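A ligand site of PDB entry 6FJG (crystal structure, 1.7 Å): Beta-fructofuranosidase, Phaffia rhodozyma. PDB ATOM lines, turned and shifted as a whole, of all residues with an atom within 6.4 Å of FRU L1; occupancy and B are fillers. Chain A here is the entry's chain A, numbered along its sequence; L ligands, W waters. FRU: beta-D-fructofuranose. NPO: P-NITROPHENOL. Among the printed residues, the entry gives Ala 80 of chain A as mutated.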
ATOM      1  N   TRP A  77       1.090  10.186  11.479  1.00  0.00           N
ATOM      2  CA  TRP A  77       2.218  10.942  11.983  1.00  0.00           C
ATOM      3  C   TRP A  77       1.925  11.446  13.399  1.00  0.00           C
ATOM      4  O   TRP A  77       0.860  11.998  13.651  1.00  0.00           O
ATOM      5  CB  TRP A  77       2.480  12.158  11.082  1.00  0.00           C
ATOM      6  CG  TRP A  77       3.456  13.096  11.662  1.00  0.00           C
ATOM      7  CD1 TRP A  77       3.183  14.128  12.521  1.00  0.00           C
ATOM      8  CD2 TRP A  77       4.872  13.065  11.534  1.00  0.00           C
ATOM      9  NE1 TRP A  77       4.333  14.750  12.906  1.00  0.00           N
ATOM     10  CE2 TRP A  77       5.387  14.120  12.307  1.00  0.00           C
ATOM     11  CE3 TRP A  77       5.761  12.250  10.822  1.00  0.00           C
ATOM     12  CZ2 TRP A  77       6.761  14.374  12.395  1.00  0.00           C
ATOM     13  CZ3 TRP A  77       7.127  12.508  10.920  1.00  0.00           C
ATOM     14  CH2 TRP A  77       7.606  13.558  11.694  1.00  0.00           C
ATOM     15  N   ASN A  79       4.304  13.677  16.608  1.00  0.00           N
ATOM     16  CA  ASN A  79       5.545  14.180  17.166  1.00  0.00           C
ATOM     17  C   ASN A  79       5.385  14.548  18.652  1.00  0.00           C
ATOM     18  O   ASN A  79       5.025  13.676  19.440  1.00  0.00           O
ATOM     19  CB  ASN A  79       6.301  15.191  16.244  1.00  0.00           C
ATOM     20  CG  ASN A  79       5.522  16.441  15.878  1.00  0.00           C
ATOM     21  OD1 ASN A  79       4.526  16.406  15.163  1.00  0.00           O
ATOM     22  ND2 ASN A  79       6.031  17.591  16.331  1.00  0.00           N
ATOM     23  N   ALA A  80       5.654  15.796  19.034  1.00  0.00           N
ATOM     24  CA  ALA A  80       5.817  16.197  20.444  1.00  0.00           C
ATOM     25  C   ALA A  80       4.613  15.899  21.328  1.00  0.00           C
ATOM     26  O   ALA A  80       3.484  16.186  20.931  1.00  0.00           O
ATOM     27  CB  ALA A  80       6.071  17.690  20.528  1.00  0.00           C
ATOM     28  N   GLN A  97       1.202  16.147  19.208  1.00  0.00           N
ATOM     29  CA  GLN A  97       1.173  16.674  17.844  1.00  0.00           C
ATOM     30  C   GLN A  97       0.860  15.532  16.887  1.00  0.00           C
ATOM     31  O   GLN A  97       1.538  14.503  16.895  1.00  0.00           O
ATOM     32  CB  GLN A  97       2.507  17.323  17.497  1.00  0.00           C
ATOM     33  CG  GLN A  97       2.823  18.564  18.334  1.00  0.00           C
ATOM     34  CD  GLN A  97       2.120  19.802  17.820  1.00  0.00           C
ATOM     35  OE1 GLN A  97       2.605  20.444  16.885  1.00  0.00           O
ATOM     36  NE2 GLN A  97       0.978  20.144  18.425  1.00  0.00           N
ATOM     37  N   TRP A 105       4.594  15.445   8.684  1.00  0.00           N
ATOM     38  CA  TRP A 105       4.008  16.533   9.482  1.00  0.00           C
ATOM     39  C   TRP A 105       3.097  17.430   8.644  1.00  0.00           C
ATOM     40  O   TRP A 105       3.315  17.625   7.444  1.00  0.00           O
ATOM     41  CB  TRP A 105       5.161  17.345  10.064  1.00  0.00           C
ATOM     42  CG  TRP A 105       4.853  18.487  10.974  1.00  0.00           C
ATOM     43  CD1 TRP A 105       4.877  18.464  12.343  1.00  0.00           C
ATOM     44  CD2 TRP A 105       4.590  19.838  10.598  1.00  0.00           C
ATOM     45  NE1 TRP A 105       4.610  19.712  12.846  1.00  0.00           N
ATOM     46  CE2 TRP A 105       4.434  20.577  11.793  1.00  0.00           C
ATOM     47  CE3 TRP A 105       4.457  20.500   9.371  1.00  0.00           C
ATOM     48  CZ2 TRP A 105       4.156  21.944  11.790  1.00  0.00           C
ATOM     49  CZ3 TRP A 105       4.172  21.863   9.372  1.00  0.00           C
ATOM     50  CH2 TRP A 105       4.036  22.573  10.574  1.00  0.00           C
ATOM     51  N   ILE A 108      -1.089  20.449  11.797  1.00  0.00           N
ATOM     52  CA  ILE A 108      -0.766  19.758  13.035  1.00  0.00           C
ATOM     53  C   ILE A 108      -1.827  20.064  14.104  1.00  0.00           C
ATOM     54  O   ILE A 108      -2.294  21.190  14.226  1.00  0.00           O
ATOM     55  CB  ILE A 108       0.706  19.994  13.456  1.00  0.00           C
ATOM     56  CG1 ILE A 108       1.222  18.828  14.302  1.00  0.00           C
ATOM     57  CG2 ILE A 108       0.884  21.336  14.155  1.00  0.00           C
ATOM     58  CD1 ILE A 108       1.478  17.533  13.508  1.00  0.00           C
ATOM     59  N   VAL A 144      -1.821  23.895  15.062  1.00  0.00           N
ATOM     60  CA  VAL A 144      -1.936  23.979  16.520  1.00  0.00           C
ATOM     61  C   VAL A 144      -0.677  23.316  17.056  1.00  0.00           C
ATOM     62  O   VAL A 144      -0.608  22.090  17.130  1.00  0.00           O
ATOM     63  CB  VAL A 144      -3.210  23.266  16.999  1.00  0.00           C
ATOM     64  CG1 VAL A 144      -3.271  23.161  18.519  1.00  0.00           C
ATOM     65  CG2 VAL A 144      -4.427  24.002  16.475  1.00  0.00           C
ATOM     66  N   PHE A 145       0.311  24.139  17.383  1.00  0.00           N
ATOM     67  CA  PHE A 145       1.616  23.683  17.848  1.00  0.00           C
ATOM     68  C   PHE A 145       1.529  23.326  19.339  1.00  0.00           C
ATOM     69  O   PHE A 145       0.432  23.295  19.914  1.00  0.00           O
ATOM     70  CB  PHE A 145       2.670  24.783  17.581  1.00  0.00           C
ATOM     71  CG  PHE A 145       3.231  24.818  16.163  1.00  0.00           C
ATOM     72  CD1 PHE A 145       2.456  24.480  15.056  1.00  0.00           C
ATOM     73  CD2 PHE A 145       4.537  25.230  15.956  1.00  0.00           C
ATOM     74  CE1 PHE A 145       2.984  24.576  13.779  1.00  0.00           C
ATOM     75  CE2 PHE A 145       5.072  25.314  14.679  1.00  0.00           C
ATOM     76  CZ  PHE A 145       4.295  24.975  13.590  1.00  0.00           C
ATOM     77  N   ASP A 146       2.673  23.046  19.949  1.00  0.00           N
ATOM     78  CA  ASP A 146       2.740  22.631  21.356  1.00  0.00           C
ATOM     79  C   ASP A 146       2.085  23.646  22.297  1.00  0.00           C
ATOM     80  O   ASP A 146       2.037  24.845  22.007  1.00  0.00           O
ATOM     81  CB  ASP A 146       4.233  22.472  21.707  1.00  0.00           C
ATOM     82  CG  ASP A 146       4.499  21.838  23.059  1.00  0.00           C
ATOM     83  OD1 ASP A 146       3.619  21.229  23.698  1.00  0.00           O
ATOM     84  OD2 ASP A 146       5.693  21.946  23.473  1.00  0.00           O
ATOM     85  N   GLY A 147       1.577  23.154  23.410  1.00  0.00           N
ATOM     86  CA  GLY A 147       0.986  23.977  24.449  1.00  0.00           C
ATOM     87  C   GLY A 147       0.949  23.225  25.763  1.00  0.00           C
ATOM     88  O   GLY A 147       1.208  22.026  25.812  1.00  0.00           O
ATOM     89  N   THR A 163       0.742  27.383  21.009  1.00  0.00           N
ATOM     90  CA  THR A 163       1.196  28.179  19.884  1.00  0.00           C
ATOM     91  C   THR A 163       0.255  28.007  18.698  1.00  0.00           C
ATOM     92  O   THR A 163       0.133  26.917  18.126  1.00  0.00           O
ATOM     93  CB  THR A 163       2.646  27.867  19.486  1.00  0.00           C
ATOM     94  OG1 THR A 163       3.515  28.202  20.576  1.00  0.00           O
ATOM     95  CG2 THR A 163       3.041  28.671  18.265  1.00  0.00           C
ATOM     96  N   ARG A 220       7.608  30.086  20.346  1.00  0.00           N
ATOM     97  CA  ARG A 220       6.620  29.016  20.490  1.00  0.00           C
ATOM     98  C   ARG A 220       6.806  28.189  21.734  1.00  0.00           C
ATOM     99  O   ARG A 220       7.785  28.352  22.480  1.00  0.00           O
ATOM    100  CB  ARG A 220       6.626  28.117  19.233  1.00  0.00           C
ATOM    101  CG  ARG A 220       7.951  27.439  18.900  1.00  0.00           C
ATOM    102  CD  ARG A 220       7.756  26.382  17.807  1.00  0.00           C
ATOM    103  NE  ARG A 220       9.017  25.961  17.217  1.00  0.00           N
ATOM    104  CZ  ARG A 220       9.740  26.651  16.317  1.00  0.00           C
ATOM    105  NH1 ARG A 220       9.341  27.843  15.881  1.00  0.00           N
ATOM    106  NH2 ARG A 220      10.894  26.167  15.884  1.00  0.00           N
ATOM    107  N   ASP A 221       5.832  27.299  21.947  1.00  0.00           N
ATOM    108  CA  ASP A 221       5.875  26.259  22.973  1.00  0.00           C
ATOM    109  C   ASP A 221       5.740  26.855  24.377  1.00  0.00           C
ATOM    110  O   ASP A 221       6.618  26.665  25.221  1.00  0.00           O
ATOM    111  CB  ASP A 221       7.128  25.399  22.850  1.00  0.00           C
ATOM    112  CG  ASP A 221       7.313  24.824  21.444  1.00  0.00           C
ATOM    113  OD1 ASP A 221       6.313  24.788  20.699  1.00  0.00           O
ATOM    114  OD2 ASP A 221       8.450  24.445  21.086  1.00  0.00           O
ATOM    115  N   PHE A 302      15.750  27.513  20.762  1.00  0.00           N
ATOM    116  CA  PHE A 302      15.152  26.535  21.678  1.00  0.00           C
ATOM    117  C   PHE A 302      13.770  26.130  21.221  1.00  0.00           C
ATOM    118  O   PHE A 302      13.040  26.935  20.627  1.00  0.00           O
ATOM    119  CB  PHE A 302      15.001  27.089  23.099  1.00  0.00           C
ATOM    120  CG  PHE A 302      16.292  27.326  23.858  1.00  0.00           C
ATOM    121  CD1 PHE A 302      17.413  26.529  23.658  1.00  0.00           C
ATOM    122  CD2 PHE A 302      16.349  28.337  24.800  1.00  0.00           C
ATOM    123  CE1 PHE A 302      18.589  26.765  24.372  1.00  0.00           C
ATOM    124  CE2 PHE A 302      17.517  28.576  25.525  1.00  0.00           C
ATOM    125  CZ  PHE A 302      18.624  27.779  25.323  1.00  0.00           C
ATOM    126  N   GLU A 303      13.406  24.898  21.547  1.00  0.00           N
ATOM    127  CA  GLU A 303      12.041  24.379  21.386  1.00  0.00           C
ATOM    128  C   GLU A 303      11.641  23.614  22.639  1.00  0.00           C
ATOM    129  O   GLU A 303      12.492  23.074  23.352  1.00  0.00           O
ATOM    130  CB  GLU A 303      11.929  23.469  20.159  1.00  0.00           C
ATOM    131  CG  GLU A 303      12.252  24.158  18.832  1.00  0.00           C
ATOM    132  CD  GLU A 303      12.092  23.236  17.643  1.00  0.00           C
ATOM    133  OE1 GLU A 303      12.813  22.216  17.599  1.00  0.00           O
ATOM    134  OE2 GLU A 303      11.271  23.524  16.750  1.00  0.00           O
ATOM    135  N   THR A 304      10.335  23.601  22.913  1.00  0.00           N
ATOM    136  CA  THR A 304       9.715  22.831  24.001  1.00  0.00           C
ATOM    137  C   THR A 304      10.412  22.969  25.356  1.00  0.00           C
ATOM    138  O   THR A 304      10.546  21.982  26.077  1.00  0.00           O
ATOM    139  CB  THR A 304       9.504  21.314  23.652  1.00  0.00           C
ATOM    140  OG1 THR A 304      10.748  20.604  23.709  1.00  0.00           O
ATOM    141  CG2 THR A 304       8.880  21.138  22.274  1.00  0.00           C
ATOM    142  N   HIS A 343      18.960  17.948  16.332  1.00  0.00           N
ATOM    143  CA  HIS A 343      18.218  18.201  17.568  1.00  0.00           C
ATOM    144  C   HIS A 343      18.862  17.590  18.814  1.00  0.00           C
ATOM    145  O   HIS A 343      19.159  16.389  18.839  1.00  0.00           O
ATOM    146  CB  HIS A 343      16.806  17.631  17.432  1.00  0.00           C
ATOM    147  CG  HIS A 343      15.906  18.437  16.564  1.00  0.00           C
ATOM    148  ND1 HIS A 343      14.839  17.888  15.880  1.00  0.00           N
ATOM    149  CD2 HIS A 343      15.919  19.760  16.257  1.00  0.00           C
ATOM    150  CE1 HIS A 343      14.229  18.844  15.198  1.00  0.00           C
ATOM    151  NE2 HIS A 343      14.864  19.978  15.403  1.00  0.00           N
ATOM    152  N   TYR A 376      13.335  13.662  21.317  1.00  0.00           N
ATOM    153  CA  TYR A 376      13.280  15.116  21.362  1.00  0.00           C
ATOM    154  C   TYR A 376      11.941  15.533  21.947  1.00  0.00           C
ATOM    155  O   TYR A 376      11.048  14.706  22.140  1.00  0.00           O
ATOM    156  CB  TYR A 376      13.429  15.656  19.941  1.00  0.00           C
ATOM    157  CG  TYR A 376      13.718  17.146  19.813  1.00  0.00           C
ATOM    158  CD1 TYR A 376      14.859  17.714  20.374  1.00  0.00           C
ATOM    159  CD2 TYR A 376      12.857  17.974  19.081  1.00  0.00           C
ATOM    160  CE1 TYR A 376      15.143  19.054  20.222  1.00  0.00           C
ATOM    161  CE2 TYR A 376      13.126  19.322  18.934  1.00  0.00           C
ATOM    162  CZ  TYR A 376      14.273  19.868  19.505  1.00  0.00           C
ATOM    163  OH  TYR A 376      14.555  21.200  19.364  1.00  0.00           O
ATOM    164  N   ALA A 377      11.797  16.829  22.219  1.00  0.00           N
ATOM    165  CA  ALA A 377      10.517  17.419  22.586  1.00  0.00           C
ATOM    166  C   ALA A 377       9.988  16.881  23.909  1.00  0.00           C
ATOM    167  O   ALA A 377       8.822  16.542  24.029  1.00  0.00           O
ATOM    168  CB  ALA A 377       9.487  17.253  21.476  1.00  0.00           C
ATOM    169  N   TRP A 393       9.334  12.375  22.647  1.00  0.00           N
ATOM    170  CA  TRP A 393       8.978  11.724  21.390  1.00  0.00           C
ATOM    171  C   TRP A 393      10.193  11.039  20.813  1.00  0.00           C
ATOM    172  O   TRP A 393      11.264  11.642  20.725  1.00  0.00           O
ATOM    173  CB  TRP A 393       8.448  12.784  20.434  1.00  0.00           C
ATOM    174  CG  TRP A 393       8.516  12.534  18.950  1.00  0.00           C
ATOM    175  CD1 TRP A 393       7.893  11.564  18.234  1.00  0.00           C
ATOM    176  CD2 TRP A 393       9.188  13.358  18.008  1.00  0.00           C
ATOM    177  NE1 TRP A 393       8.160  11.723  16.880  1.00  0.00           N
ATOM    178  CE2 TRP A 393       8.957  12.820  16.724  1.00  0.00           C
ATOM    179  CE3 TRP A 393       9.984  14.512  18.131  1.00  0.00           C
ATOM    180  CZ2 TRP A 393       9.479  13.403  15.567  1.00  0.00           C
ATOM    181  CZ3 TRP A 393      10.527  15.074  16.970  1.00  0.00           C
ATOM    182  CH2 TRP A 393      10.271  14.522  15.716  1.00  0.00           C
HETATM  183  C1  FRU L   1       9.395  20.402  18.445  1.00  0.00           C
HETATM  184  C2  FRU L   1       8.352  21.263  17.743  1.00  0.00           C
HETATM  185  C3  FRU L   1       7.802  22.347  18.645  1.00  0.00           C
HETATM  186  C4  FRU L   1       6.502  22.692  17.920  1.00  0.00           C
HETATM  187  C5  FRU L   1       6.046  21.345  17.383  1.00  0.00           C
HETATM  188  C6  FRU L   1       5.395  21.471  16.014  1.00  0.00           C
HETATM  189  O1  FRU L   1       9.927  19.438  17.521  1.00  0.00           O
HETATM  190  O2  FRU L   1       8.912  21.843  16.562  1.00  0.00           O
HETATM  191  O3  FRU L   1       8.728  23.437  18.752  1.00  0.00           O
HETATM  192  O4  FRU L   1       5.484  23.229  18.780  1.00  0.00           O
HETATM  193  O5  FRU L   1       7.211  20.507  17.331  1.00  0.00           O
HETATM  194  O6  FRU L   1       4.791  20.225  15.570  1.00  0.00           O
HETATM  195  C1  NPO L   2       7.664  22.993  11.094  1.00  0.00           C
HETATM  196  C2  NPO L   2       7.926  23.532  12.364  1.00  0.00           C
HETATM  197  C3  NPO L   2       8.207  22.679  13.432  1.00  0.00           C
HETATM  198  C4  NPO L   2       8.232  21.289  13.242  1.00  0.00           C
HETATM  199  C5  NPO L   2       7.971  20.750  11.971  1.00  0.00           C
HETATM  200  C6  NPO L   2       7.690  21.604  10.904  1.00  0.00           C
HETATM  201  OH  NPO L   2       8.511  20.443  14.269  1.00  0.00           O
HETATM  202  N1  NPO L   2       7.365  23.829   9.999  1.00  0.00           N
HETATM  203  O2  NPO L   2       7.163  23.291   8.719  1.00  0.00           O
HETATM  204  O3  NPO L   2       7.290  25.050  10.134  1.00  0.00           O
HETATM  205  O   HOH W   1      11.665  20.423  15.764  1.00  0.00           O
HETATM  206  O   HOH W   2       8.513  17.346  17.824  1.00  0.00           O
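Water W2 lies within hydrogen-bond range of O1 of FRU L1 (2.5 Å), ND2 of Asn 79 (2.9 Å) and N of Ala 80 (3.5 Å).
Water W1 lies within hydrogen-bond range of an oxygen (O1) of FRU L1 (2.7 Å), the side-chain carboxylate of Glu 303 (2.8 Å), a ring nitrogen (NE2) of His 343 (3.2 Å) and an oxygen (OH) of NPO L2 (3.5 Å).
Residues that only touch FRU L1: Phe 145 (3.4 Å), Thr 304 (3.9 Å) and Tyr 376 (3.5 Å).
Hydrophobic or aromatic side chains within 4 Å of FRU L1: Trp 105, Phe 145 and Tyr 376.
Ten residues have an atom within 4 Å of FRU L1: Asn 79, Gln 97, Trp 105, Phe 145, Asp 146, Arg 220, Asp 221, Glu 303, Thr 304 and Tyr 376.
The side-chain hydroxyl (OG1) of Thr 163 sits at hydrogen-bond distance from the backbone NH (N) of Asp 221 (2.8 Å).
The backbone carbonyl oxygen of Gln 97 is in hydrogen-bond range of the backbone NH of Asn 79, at 2.9 Å.
The backbone NH of Gln 97 lies within hydrogen-bond range of the backbone carbonyl oxygen of Ala 80, at 2.9 Å.
The side-chain carboxylate of Glu 303 is in salt-bridge range of the guanidinium group of Arg 220, at 2.8 Å.
OE1 of Glu 303 is in hydrogen-bond range of OH of Tyr 376 (2.7 Å).
The indole nitrogen of Trp 77 lies within hydrogen-bond range of the side-chain amide oxygen of Asn 79, at 2.8 Å.
O of Asp 146 sits at hydrogen-bond distance from N of Thr 163, 3.0 Å away.
The backbone NH (N) of Phe 145 is in hydrogen-bond range of the backbone carbonyl oxygen (O) of Thr 163, at 2.9 Å.
OD2 of Asp 221 is in hydrogen-bond range of O3 of FRU L1, at 2.6 Å.
The side-chain amide oxygen of Gln 97 is in hydrogen-bond range of an oxygen (O6) of FRU L1 (2.6 Å).
O6 of FRU L1 is in hydrogen-bond range of NE1 of Trp 105, at 2.8 Å.
An oxygen (O2) of FRU L1 is in hydrogen-bond range of the side-chain carboxylate (OE2) of Glu 303 (2.9 Å).
The guanidinium group (NE) of Arg 220 is in hydrogen-bond range of an oxygen (O3) of FRU L1, 3.0 Å away.
The side-chain amide nitrogen (ND2) of Asn 79 sits at hydrogen-bond distance from an oxygen (O6) of FRU L1, 3.0 Å away.
N of Asp 146 lies within hydrogen-bond range of O4 of FRU L1.
An oxygen (O2) of FRU L1 is in hydrogen-bond range of an oxygen (OH) of NPO L2.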
